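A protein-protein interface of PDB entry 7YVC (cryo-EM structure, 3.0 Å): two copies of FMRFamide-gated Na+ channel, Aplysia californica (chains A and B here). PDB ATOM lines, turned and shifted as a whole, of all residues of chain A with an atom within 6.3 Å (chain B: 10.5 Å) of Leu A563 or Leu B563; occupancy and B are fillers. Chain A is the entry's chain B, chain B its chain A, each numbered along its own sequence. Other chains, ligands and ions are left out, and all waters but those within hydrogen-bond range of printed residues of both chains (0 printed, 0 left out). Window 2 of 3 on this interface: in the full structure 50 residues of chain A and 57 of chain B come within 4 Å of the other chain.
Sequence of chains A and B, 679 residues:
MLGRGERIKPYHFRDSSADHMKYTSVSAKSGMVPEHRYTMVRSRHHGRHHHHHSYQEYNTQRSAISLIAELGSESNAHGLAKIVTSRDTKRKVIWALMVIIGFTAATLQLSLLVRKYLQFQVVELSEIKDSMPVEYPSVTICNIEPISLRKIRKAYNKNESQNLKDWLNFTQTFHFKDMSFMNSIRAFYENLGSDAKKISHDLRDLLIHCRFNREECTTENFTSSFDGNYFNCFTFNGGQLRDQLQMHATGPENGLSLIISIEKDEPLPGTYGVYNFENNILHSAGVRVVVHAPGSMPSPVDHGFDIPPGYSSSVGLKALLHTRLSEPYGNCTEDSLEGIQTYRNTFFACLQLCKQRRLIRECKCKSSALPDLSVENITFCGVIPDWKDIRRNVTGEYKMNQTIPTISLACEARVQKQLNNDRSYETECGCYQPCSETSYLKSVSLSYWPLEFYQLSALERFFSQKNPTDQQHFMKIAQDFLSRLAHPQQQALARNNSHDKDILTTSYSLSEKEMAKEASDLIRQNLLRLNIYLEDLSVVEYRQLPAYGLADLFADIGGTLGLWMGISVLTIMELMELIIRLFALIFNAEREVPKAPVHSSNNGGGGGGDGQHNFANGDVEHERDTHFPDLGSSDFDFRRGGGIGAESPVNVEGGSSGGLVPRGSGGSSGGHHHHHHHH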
ATOM      1  N   MET A  98       9.794  37.524   1.369  1.00  0.00           N
ATOM      2  CA  MET A  98       8.965  36.683   0.531  1.00  0.00           C
ATOM      3  C   MET A  98       9.003  35.225   0.965  1.00  0.00           C
ATOM      4  O   MET A  98       8.068  34.475   0.663  1.00  0.00           O
ATOM      5  CB  MET A  98       9.423  36.824  -0.917  1.00  0.00           C
ATOM      6  CG  MET A  98       8.510  36.126  -1.841  1.00  0.00           C
ATOM      7  SD  MET A  98       6.998  37.070  -1.669  1.00  0.00           S
ATOM      8  CE  MET A  98       5.846  35.830  -2.167  1.00  0.00           C
ATOM      9  N   GLY A 102       5.494  33.135   2.958  1.00  0.00           N
ATOM     10  CA  GLY A 102       5.160  31.737   2.753  1.00  0.00           C
ATOM     11  C   GLY A 102       5.158  30.954   4.051  1.00  0.00           C
ATOM     12  O   GLY A 102       4.344  30.048   4.243  1.00  0.00           O
ATOM     13  N   ALA A 105       1.874  31.659   5.643  1.00  0.00           N
ATOM     14  CA  ALA A 105       0.819  30.898   4.981  1.00  0.00           C
ATOM     15  C   ALA A 105       0.834  29.435   5.417  1.00  0.00           C
ATOM     16  O   ALA A 105      -0.222  28.838   5.669  1.00  0.00           O
ATOM     17  CB  ALA A 105       0.963  31.011   3.465  1.00  0.00           C
ATOM     18  N   GLY A 558       2.294  16.137   7.020  1.00  0.00           N
ATOM     19  CA  GLY A 558       3.638  15.670   6.736  1.00  0.00           C
ATOM     20  C   GLY A 558       4.259  16.274   5.496  1.00  0.00           C
ATOM     21  O   GLY A 558       5.489  16.328   5.397  1.00  0.00           O
ATOM     22  N   GLY A 559       3.444  16.725   4.545  1.00  0.00           N
ATOM     23  CA  GLY A 559       3.998  17.380   3.374  1.00  0.00           C
ATOM     24  C   GLY A 559       4.705  18.678   3.714  1.00  0.00           C
ATOM     25  O   GLY A 559       5.802  18.948   3.221  1.00  0.00           O
ATOM     26  N   THR A 560       4.093  19.491   4.570  1.00  0.00           N
ATOM     27  CA  THR A 560       4.642  20.795   4.903  1.00  0.00           C
ATOM     28  C   THR A 560       5.572  20.772   6.109  1.00  0.00           C
ATOM     29  O   THR A 560       6.386  21.695   6.260  1.00  0.00           O
ATOM     30  CB  THR A 560       3.504  21.789   5.155  1.00  0.00           C
ATOM     31  OG1 THR A 560       4.045  23.100   5.350  1.00  0.00           O
ATOM     32  CG2 THR A 560       2.714  21.390   6.377  1.00  0.00           C
ATOM     33  N   LEU A 561       5.482  19.740   6.954  1.00  0.00           N
ATOM     34  CA  LEU A 561       6.254  19.720   8.194  1.00  0.00           C
ATOM     35  C   LEU A 561       7.738  19.926   7.935  1.00  0.00           C
ATOM     36  O   LEU A 561       8.324  20.932   8.355  1.00  0.00           O
ATOM     37  CB  LEU A 561       6.041  18.397   8.929  1.00  0.00           C
ATOM     38  CG  LEU A 561       4.854  18.288   9.879  1.00  0.00           C
ATOM     39  CD1 LEU A 561       4.679  16.856  10.362  1.00  0.00           C
ATOM     40  CD2 LEU A 561       5.021  19.235  11.054  1.00  0.00           C
ATOM     41  N   GLY A 562       8.361  18.971   7.245  1.00  0.00           N
ATOM     42  CA  GLY A 562       9.806  18.999   7.106  1.00  0.00           C
ATOM     43  C   GLY A 562      10.291  20.236   6.381  1.00  0.00           C
ATOM     44  O   GLY A 562      11.197  20.928   6.850  1.00  0.00           O
ATOM     45  N   LEU A 563       9.653  20.562   5.255  1.00  0.00           N
ATOM     46  CA  LEU A 563      10.097  21.698   4.457  1.00  0.00           C
ATOM     47  C   LEU A 563      10.024  22.993   5.254  1.00  0.00           C
ATOM     48  O   LEU A 563      10.991  23.764   5.297  1.00  0.00           O
ATOM     49  CB  LEU A 563       9.261  21.810   3.183  1.00  0.00           C
ATOM     50  CG  LEU A 563       9.637  22.990   2.282  1.00  0.00           C
ATOM     51  CD1 LEU A 563      11.019  22.795   1.678  1.00  0.00           C
ATOM     52  CD2 LEU A 563       8.595  23.208   1.197  1.00  0.00           C
ATOM     53  N   TRP A 564       8.900  23.241   5.931  1.00  0.00           N
ATOM     54  CA  TRP A 564       8.765  24.560   6.530  1.00  0.00           C
ATOM     55  C   TRP A 564       9.463  24.683   7.870  1.00  0.00           C
ATOM     56  O   TRP A 564       9.971  25.766   8.185  1.00  0.00           O
ATOM     57  CB  TRP A 564       7.298  24.954   6.631  1.00  0.00           C
ATOM     58  CG  TRP A 564       6.880  25.579   5.363  1.00  0.00           C
ATOM     59  CD1 TRP A 564       6.022  25.079   4.436  1.00  0.00           C
ATOM     60  CD2 TRP A 564       7.366  26.816   4.840  1.00  0.00           C
ATOM     61  NE1 TRP A 564       5.916  25.948   3.376  1.00  0.00           N
ATOM     62  CE2 TRP A 564       6.735  27.022   3.602  1.00  0.00           C
ATOM     63  CE3 TRP A 564       8.263  27.781   5.310  1.00  0.00           C
ATOM     64  CZ2 TRP A 564       6.971  28.152   2.825  1.00  0.00           C
ATOM     65  CZ3 TRP A 564       8.499  28.898   4.538  1.00  0.00           C
ATOM     66  CH2 TRP A 564       7.856  29.076   3.311  1.00  0.00           C
ATOM     67  N   MET A 565       9.561  23.621   8.667  1.00  0.00           N
ATOM     68  CA  MET A 565      10.360  23.808   9.870  1.00  0.00           C
ATOM     69  C   MET A 565      11.850  23.747   9.539  1.00  0.00           C
ATOM     70  O   MET A 565      12.670  24.304  10.275  1.00  0.00           O
ATOM     71  CB  MET A 565       9.932  22.835  10.978  1.00  0.00           C
ATOM     72  CG  MET A 565      10.051  21.350  10.749  1.00  0.00           C
ATOM     73  SD  MET A 565      11.722  20.762  10.980  1.00  0.00           S
ATOM     74  CE  MET A 565      11.918  20.911  12.756  1.00  0.00           C
ATOM     75  N   GLY A 566      12.216  23.180   8.383  1.00  0.00           N
ATOM     76  CA  GLY A 566      13.571  23.366   7.884  1.00  0.00           C
ATOM     77  C   GLY A 566      13.857  24.803   7.493  1.00  0.00           C
ATOM     78  O   GLY A 566      14.917  25.350   7.816  1.00  0.00           O
ATOM     79  N   ILE A 567      12.919  25.431   6.776  1.00  0.00           N
ATOM     80  CA  ILE A 567      13.064  26.850   6.451  1.00  0.00           C
ATOM     81  C   ILE A 567      13.175  27.674   7.727  1.00  0.00           C
ATOM     82  O   ILE A 567      13.995  28.600   7.823  1.00  0.00           O
ATOM     83  CB  ILE A 567      11.891  27.329   5.574  1.00  0.00           C
ATOM     84  CG1 ILE A 567      11.866  26.587   4.240  1.00  0.00           C
ATOM     85  CG2 ILE A 567      11.986  28.822   5.330  1.00  0.00           C
ATOM     86  CD1 ILE A 567      13.156  26.690   3.460  1.00  0.00           C
ATOM     87  N   SER A 568      12.352  27.349   8.727  1.00  0.00           N
ATOM     88  CA  SER A 568      12.403  28.067   9.996  1.00  0.00           C
ATOM     89  C   SER A 568      13.755  27.897  10.677  1.00  0.00           C
ATOM     90  O   SER A 568      14.319  28.868  11.195  1.00  0.00           O
ATOM     91  CB  SER A 568      11.274  27.593  10.912  1.00  0.00           C
ATOM     92  OG  SER A 568      11.679  26.474  11.682  1.00  0.00           O
ATOM     93  N   VAL B  99      12.303  23.487 -11.968  1.00  0.00           N
ATOM     94  CA  VAL B  99      11.464  24.323 -11.117  1.00  0.00           C
ATOM     95  C   VAL B  99      10.135  24.634 -11.795  1.00  0.00           C
ATOM     96  O   VAL B  99       9.077  24.607 -11.154  1.00  0.00           O
ATOM     97  CB  VAL B  99      12.226  25.610 -10.738  1.00  0.00           C
ATOM     98  CG1 VAL B  99      11.265  26.697 -10.287  1.00  0.00           C
ATOM     99  CG2 VAL B  99      13.246  25.319  -9.652  1.00  0.00           C
ATOM    100  N   GLY B 102       7.560  21.849 -11.561  1.00  0.00           N
ATOM    101  CA  GLY B 102       6.900  21.883 -10.266  1.00  0.00           C
ATOM    102  C   GLY B 102       5.887  23.006 -10.172  1.00  0.00           C
ATOM    103  O   GLY B 102       4.835  22.858  -9.544  1.00  0.00           O
ATOM    104  N   PHE B 103       6.189  24.145 -10.798  1.00  0.00           N
ATOM    105  CA  PHE B 103       5.212  25.229 -10.856  1.00  0.00           C
ATOM    106  C   PHE B 103       3.949  24.791 -11.587  1.00  0.00           C
ATOM    107  O   PHE B 103       2.832  25.095 -11.150  1.00  0.00           O
ATOM    108  CB  PHE B 103       5.816  26.455 -11.538  1.00  0.00           C
ATOM    109  CG  PHE B 103       4.808  27.520 -11.869  1.00  0.00           C
ATOM    110  CD1 PHE B 103       4.393  28.420 -10.906  1.00  0.00           C
ATOM    111  CD2 PHE B 103       4.274  27.618 -13.142  1.00  0.00           C
ATOM    112  CE1 PHE B 103       3.467  29.397 -11.204  1.00  0.00           C
ATOM    113  CE2 PHE B 103       3.347  28.593 -13.447  1.00  0.00           C
ATOM    114  CZ  PHE B 103       2.943  29.483 -12.478  1.00  0.00           C
ATOM    115  N   ALA B 106       1.954  22.553  -9.303  1.00  0.00           N
ATOM    116  CA  ALA B 106       1.250  23.336  -8.293  1.00  0.00           C
ATOM    117  C   ALA B 106       0.040  24.045  -8.887  1.00  0.00           C
ATOM    118  O   ALA B 106      -1.011  24.140  -8.244  1.00  0.00           O
ATOM    119  CB  ALA B 106       2.200  24.345  -7.654  1.00  0.00           C
ATOM    120  N   THR B 107       0.175  24.564 -10.108  1.00  0.00           N
ATOM    121  CA  THR B 107      -0.957  25.211 -10.762  1.00  0.00           C
ATOM    122  C   THR B 107      -2.076  24.215 -11.036  1.00  0.00           C
ATOM    123  O   THR B 107      -3.261  24.545 -10.902  1.00  0.00           O
ATOM    124  CB  THR B 107      -0.508  25.878 -12.061  1.00  0.00           C
ATOM    125  OG1 THR B 107       0.654  26.675 -11.809  1.00  0.00           O
ATOM    126  CG2 THR B 107      -1.614  26.764 -12.605  1.00  0.00           C
ATOM    127  N   GLN B 109      -2.683  21.634  -9.164  1.00  0.00           N
ATOM    128  CA  GLN B 109      -3.307  21.417  -7.862  1.00  0.00           C
ATOM    129  C   GLN B 109      -4.270  22.548  -7.515  1.00  0.00           C
ATOM    130  O   GLN B 109      -5.382  22.302  -7.029  1.00  0.00           O
ATOM    131  CB  GLN B 109      -2.242  21.276  -6.777  1.00  0.00           C
ATOM    132  CG  GLN B 109      -2.831  21.167  -5.384  1.00  0.00           C
ATOM    133  CD  GLN B 109      -1.910  21.690  -4.307  1.00  0.00           C
ATOM    134  OE1 GLN B 109      -1.728  22.898  -4.166  1.00  0.00           O
ATOM    135  NE2 GLN B 109      -1.333  20.785  -3.530  1.00  0.00           N
ATOM    136  N   LEU B 110      -3.858  23.794  -7.759  1.00  0.00           N
ATOM    137  CA  LEU B 110      -4.732  24.931  -7.486  1.00  0.00           C
ATOM    138  C   LEU B 110      -6.010  24.850  -8.308  1.00  0.00           C
ATOM    139  O   LEU B 110      -7.113  25.043  -7.783  1.00  0.00           O
ATOM    140  CB  LEU B 110      -4.012  26.246  -7.775  1.00  0.00           C
ATOM    141  CG  LEU B 110      -2.822  26.640  -6.913  1.00  0.00           C
ATOM    142  CD1 LEU B 110      -2.190  27.895  -7.469  1.00  0.00           C
ATOM    143  CD2 LEU B 110      -3.285  26.870  -5.499  1.00  0.00           C
ATOM    144  N   ASP B 556      -6.201  23.952   2.369  1.00  0.00           N
ATOM    145  CA  ASP B 556      -5.484  23.187   1.352  1.00  0.00           C
ATOM    146  C   ASP B 556      -4.640  24.079   0.452  1.00  0.00           C
ATOM    147  O   ASP B 556      -3.591  23.645  -0.037  1.00  0.00           O
ATOM    148  CB  ASP B 556      -6.462  22.371   0.508  1.00  0.00           C
ATOM    149  CG  ASP B 556      -6.648  20.966   1.033  1.00  0.00           C
ATOM    150  OD1 ASP B 556      -5.762  20.489   1.772  1.00  0.00           O
ATOM    151  OD2 ASP B 556      -7.670  20.333   0.701  1.00  0.00           O
ATOM    152  N   ILE B 557      -5.072  25.315   0.220  1.00  0.00           N
ATOM    153  CA  ILE B 557      -4.357  26.191  -0.700  1.00  0.00           C
ATOM    154  C   ILE B 557      -3.247  26.983  -0.013  1.00  0.00           C
ATOM    155  O   ILE B 557      -2.191  27.208  -0.619  1.00  0.00           O
ATOM    156  CB  ILE B 557      -5.355  27.123  -1.407  1.00  0.00           C
ATOM    157  CG1 ILE B 557      -6.382  26.298  -2.172  1.00  0.00           C
ATOM    158  CG2 ILE B 557      -4.655  28.024  -2.381  1.00  0.00           C
ATOM    159  CD1 ILE B 557      -5.773  25.438  -3.240  1.00  0.00           C
ATOM    160  N   GLY B 558      -3.441  27.382   1.246  1.00  0.00           N
ATOM    161  CA  GLY B 558      -2.460  28.206   1.928  1.00  0.00           C
ATOM    162  C   GLY B 558      -1.085  27.584   2.028  1.00  0.00           C
ATOM    163  O   GLY B 558      -0.096  28.312   2.152  1.00  0.00           O
ATOM    164  N   GLY B 559      -0.995  26.257   1.982  1.00  0.00           N
ATOM    165  CA  GLY B 559       0.312  25.624   1.998  1.00  0.00           C
ATOM    166  C   GLY B 559       1.135  25.958   0.770  1.00  0.00           C
ATOM    167  O   GLY B 559       2.325  26.265   0.871  1.00  0.00           O
ATOM    168  N   THR B 560       0.511  25.917  -0.404  1.00  0.00           N
ATOM    169  CA  THR B 560       1.222  26.142  -1.651  1.00  0.00           C
ATOM    170  C   THR B 560       1.236  27.600  -2.088  1.00  0.00           C
ATOM    171  O   THR B 560       2.104  27.981  -2.889  1.00  0.00           O
ATOM    172  CB  THR B 560       0.610  25.282  -2.761  1.00  0.00           C
ATOM    173  OG1 THR B 560       1.395  25.402  -3.951  1.00  0.00           O
ATOM    174  CG2 THR B 560      -0.804  25.722  -3.051  1.00  0.00           C
ATOM    175  N   LEU B 561       0.315  28.422  -1.574  1.00  0.00           N
ATOM    176  CA  LEU B 561       0.194  29.798  -2.046  1.00  0.00           C
ATOM    177  C   LEU B 561       1.518  30.540  -1.957  1.00  0.00           C
ATOM    178  O   LEU B 561       2.098  30.934  -2.977  1.00  0.00           O
ATOM    179  CB  LEU B 561      -0.868  30.543  -1.238  1.00  0.00           C
ATOM    180  CG  LEU B 561      -2.318  30.449  -1.700  1.00  0.00           C
ATOM    181  CD1 LEU B 561      -3.251  31.075  -0.676  1.00  0.00           C
ATOM    182  CD2 LEU B 561      -2.489  31.107  -3.058  1.00  0.00           C
ATOM    183  N   GLY B 562       2.004  30.744  -0.733  1.00  0.00           N
ATOM    184  CA  GLY B 562       3.166  31.596  -0.546  1.00  0.00           C
ATOM    185  C   GLY B 562       4.393  31.061  -1.255  1.00  0.00           C
ATOM    186  O   GLY B 562       5.065  31.790  -1.987  1.00  0.00           O
ATOM    187  N   LEU B 563       4.665  29.766  -1.091  1.00  0.00           N
ATOM    188  CA  LEU B 563       5.862  29.183  -1.683  1.00  0.00           C
ATOM    189  C   LEU B 563       5.851  29.320  -3.198  1.00  0.00           C
ATOM    190  O   LEU B 563       6.836  29.769  -3.799  1.00  0.00           O
ATOM    191  CB  LEU B 563       5.989  27.713  -1.282  1.00  0.00           C
ATOM    192  CG  LEU B 563       7.211  27.001  -1.873  1.00  0.00           C
ATOM    193  CD1 LEU B 563       8.500  27.550  -1.279  1.00  0.00           C
ATOM    194  CD2 LEU B 563       7.120  25.496  -1.673  1.00  0.00           C
ATOM    195  N   TRP B 564       4.735  28.976  -3.843  1.00  0.00           N
ATOM    196  CA  TRP B 564       4.796  28.928  -5.295  1.00  0.00           C
ATOM    197  C   TRP B 564       4.619  30.285  -5.948  1.00  0.00           C
ATOM    198  O   TRP B 564       5.228  30.531  -6.996  1.00  0.00           O
ATOM    199  CB  TRP B 564       3.797  27.916  -5.840  1.00  0.00           C
ATOM    200  CG  TRP B 564       4.425  26.582  -5.853  1.00  0.00           C
ATOM    201  CD1 TRP B 564       4.113  25.513  -5.076  1.00  0.00           C
ATOM    202  CD2 TRP B 564       5.539  26.189  -6.656  1.00  0.00           C
ATOM    203  NE1 TRP B 564       4.947  24.460  -5.366  1.00  0.00           N
ATOM    204  CE2 TRP B 564       5.834  24.853  -6.334  1.00  0.00           C
ATOM    205  CE3 TRP B 564       6.307  26.834  -7.630  1.00  0.00           C
ATOM    206  CZ2 TRP B 564       6.863  24.149  -6.950  1.00  0.00           C
ATOM    207  CZ3 TRP B 564       7.329  26.138  -8.237  1.00  0.00           C
ATOM    208  CH2 TRP B 564       7.598  24.809  -7.899  1.00  0.00           C
ATOM    209  N   MET B 565       3.852  31.205  -5.365  1.00  0.00           N
ATOM    210  CA  MET B 565       3.848  32.515  -6.001  1.00  0.00           C
ATOM    211  C   MET B 565       5.117  33.288  -5.642  1.00  0.00           C
ATOM    212  O   MET B 565       5.527  34.182  -6.387  1.00  0.00           O
ATOM    213  CB  MET B 565       2.551  33.277  -5.695  1.00  0.00           C
ATOM    214  CG  MET B 565       2.211  33.619  -4.267  1.00  0.00           C
ATOM    215  SD  MET B 565       3.103  35.051  -3.682  1.00  0.00           S
ATOM    216  CE  MET B 565       2.320  36.372  -4.608  1.00  0.00           C
ATOM    217  N   GLY B 566       5.817  32.888  -4.574  1.00  0.00           N
ATOM    218  CA  GLY B 566       7.169  33.385  -4.369  1.00  0.00           C
ATOM    219  C   GLY B 566       8.138  32.895  -5.429  1.00  0.00           C
ATOM    220  O   GLY B 566       8.951  33.664  -5.951  1.00  0.00           O
ATOM    221  N   ILE B 567       8.074  31.598  -5.750  1.00  0.00           N
ATOM    222  CA  ILE B 567       8.894  31.066  -6.839  1.00  0.00           C
ATOM    223  C   ILE B 567       8.577  31.791  -8.139  1.00  0.00           C
ATOM    224  O   ILE B 567       9.480  32.136  -8.916  1.00  0.00           O
ATOM    225  CB  ILE B 567       8.688  29.544  -6.981  1.00  0.00           C
ATOM    226  CG1 ILE B 567       9.130  28.813  -5.715  1.00  0.00           C
ATOM    227  CG2 ILE B 567       9.453  29.014  -8.175  1.00  0.00           C
ATOM    228  CD1 ILE B 567      10.560  29.093  -5.316  1.00  0.00           C
ATOM    229  N   SER B 568       7.290  32.033  -8.396  1.00  0.00           N
ATOM    230  CA  SER B 568       6.894  32.744  -9.607  1.00  0.00           C
ATOM    231  C   SER B 568       7.458  34.160  -9.631  1.00  0.00           C
ATOM    232  O   SER B 568       7.953  34.616 -10.668  1.00  0.00           O
ATOM    233  CB  SER B 568       5.370  32.769  -9.724  1.00  0.00           C
ATOM    234  OG  SER B 568       4.823  33.889  -9.050  1.00  0.00           O
ATOM    235  N   VAL B 569       7.397  34.870  -8.501  1.00  0.00           N
ATOM    236  CA  VAL B 569       7.930  36.230  -8.447  1.00  0.00           C
ATOM    237  C   VAL B 569       9.430  36.228  -8.710  1.00  0.00           C
ATOM    238  O   VAL B 569       9.946  37.054  -9.473  1.00  0.00           O
ATOM    239  CB  VAL B 569       7.595  36.892  -7.099  1.00  0.00           C
ATOM    240  CG1 VAL B 569       8.320  38.217  -6.972  1.00  0.00           C
ATOM    241  CG2 VAL B 569       6.104  37.131  -6.996  1.00  0.00           C
ATOM    242  N   LEU B 570      10.154  35.301  -8.080  1.00  0.00           N
ATOM    243  CA  LEU B 570      11.598  35.245  -8.278  1.00  0.00           C
ATOM    244  C   LEU B 570      11.944  34.958  -9.734  1.00  0.00           C
ATOM    245  O   LEU B 570      12.803  35.629 -10.323  1.00  0.00           O
ATOM    246  CB  LEU B 570      12.214  34.188  -7.363  1.00  0.00           C
ATOM    247  CG  LEU B 570      12.051  34.408  -5.858  1.00  0.00           C
ATOM    248  CD1 LEU B 570      12.886  33.403  -5.075  1.00  0.00           C
ATOM    249  CD2 LEU B 570      12.407  35.836  -5.469  1.00  0.00           C
ATOM    250  N   THR B 571      11.268  33.980 -10.342  1.00  0.00           N
ATOM    251  CA  THR B 571      11.549  33.652 -11.735  1.00  0.00           C
ATOM    252  C   THR B 571      11.223  34.823 -12.654  1.00  0.00           C
ATOM    253  O   THR B 571      11.984  35.125 -13.582  1.00  0.00           O
ATOM    254  CB  THR B 571      10.766  32.409 -12.155  1.00  0.00           C
ATOM    255  OG1 THR B 571       9.390  32.563 -11.789  1.00  0.00           O
ATOM    256  CG2 THR B 571      11.330  31.170 -11.476  1.00  0.00           C
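O of Met B565 lies within hydrogen-bond range of OG of Ser B568.
Among the printed residues, pairs that only touch across the chains: Met A98 with Met B565 (3.2 Å), Met A98 with Gly B566 (3.5 Å), Gly A102 with Gly B562 (3.9 Å), Ala A105 with Gly B558 (3.2 Å) and Leu A563 with Leu B563 (3.96 Å).
Of chain B, only Leu B563 (3.96 Å) comes within 4 Å of Leu A563.
Leu B563 touches just one residue of chain A: Leu A563.
Of chain B, only Gly B562 (3.9 Å) comes within 4 Å of Gly A102.
No residue of chain B comes within 4 Å of Gly A562.
No residue of chain B comes within 4 Å of Trp A564.
No residue of chain B comes within 4 Å of Gly A566.
No residue of chain B comes within 4 Å of Ile A567.
Printed residues of chain A within 4 Å of Gly B566: Met A98 (3.5 Å).
Of the printed residues of chain A, Gly B558 touches Ala A105 (3.2 Å).
Of the printed residues of chain B, Met A98 touches Met B565 and Gly B566.
Printed residues of chain A within 4 Å of Gly B562: Gly A102 (3.9 Å).
Trp B564 touches none of the printed residues of chain A.
The nearest residue of chain B that does not touch Leu A563 is Gly B559 (7.0 Å).
The nearest residue of chain A that does not touch Leu B563 is Trp A564 (4.2 Å).
The nearest printed residue of chain B that does not touch Met A98 is Gly B562 (4.1 Å).
Of the 23 printed residues of chain B, 5 touch a printed residue of chain A.
Hydrophobic or aromatic side chains of chain B within 4 Å of the printed part of chain A: Leu B563 and Met B565.
Hydrophobic or aromatic side chains of chain A within 4 Å of the printed part of chain B: Met A98, Ala A105 and Leu A563.
Among the printed residues, no Asp or Glu carboxylate lies within 4 Å of a Lys or Arg side-chain nitrogen of the other chain.
Gly A102 touches Gly B562, but with the chains exchanged Gly A562 does not touch Gly B102 (17.0 Å).
Leu A563 touches its own counterpart, Leu B563.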
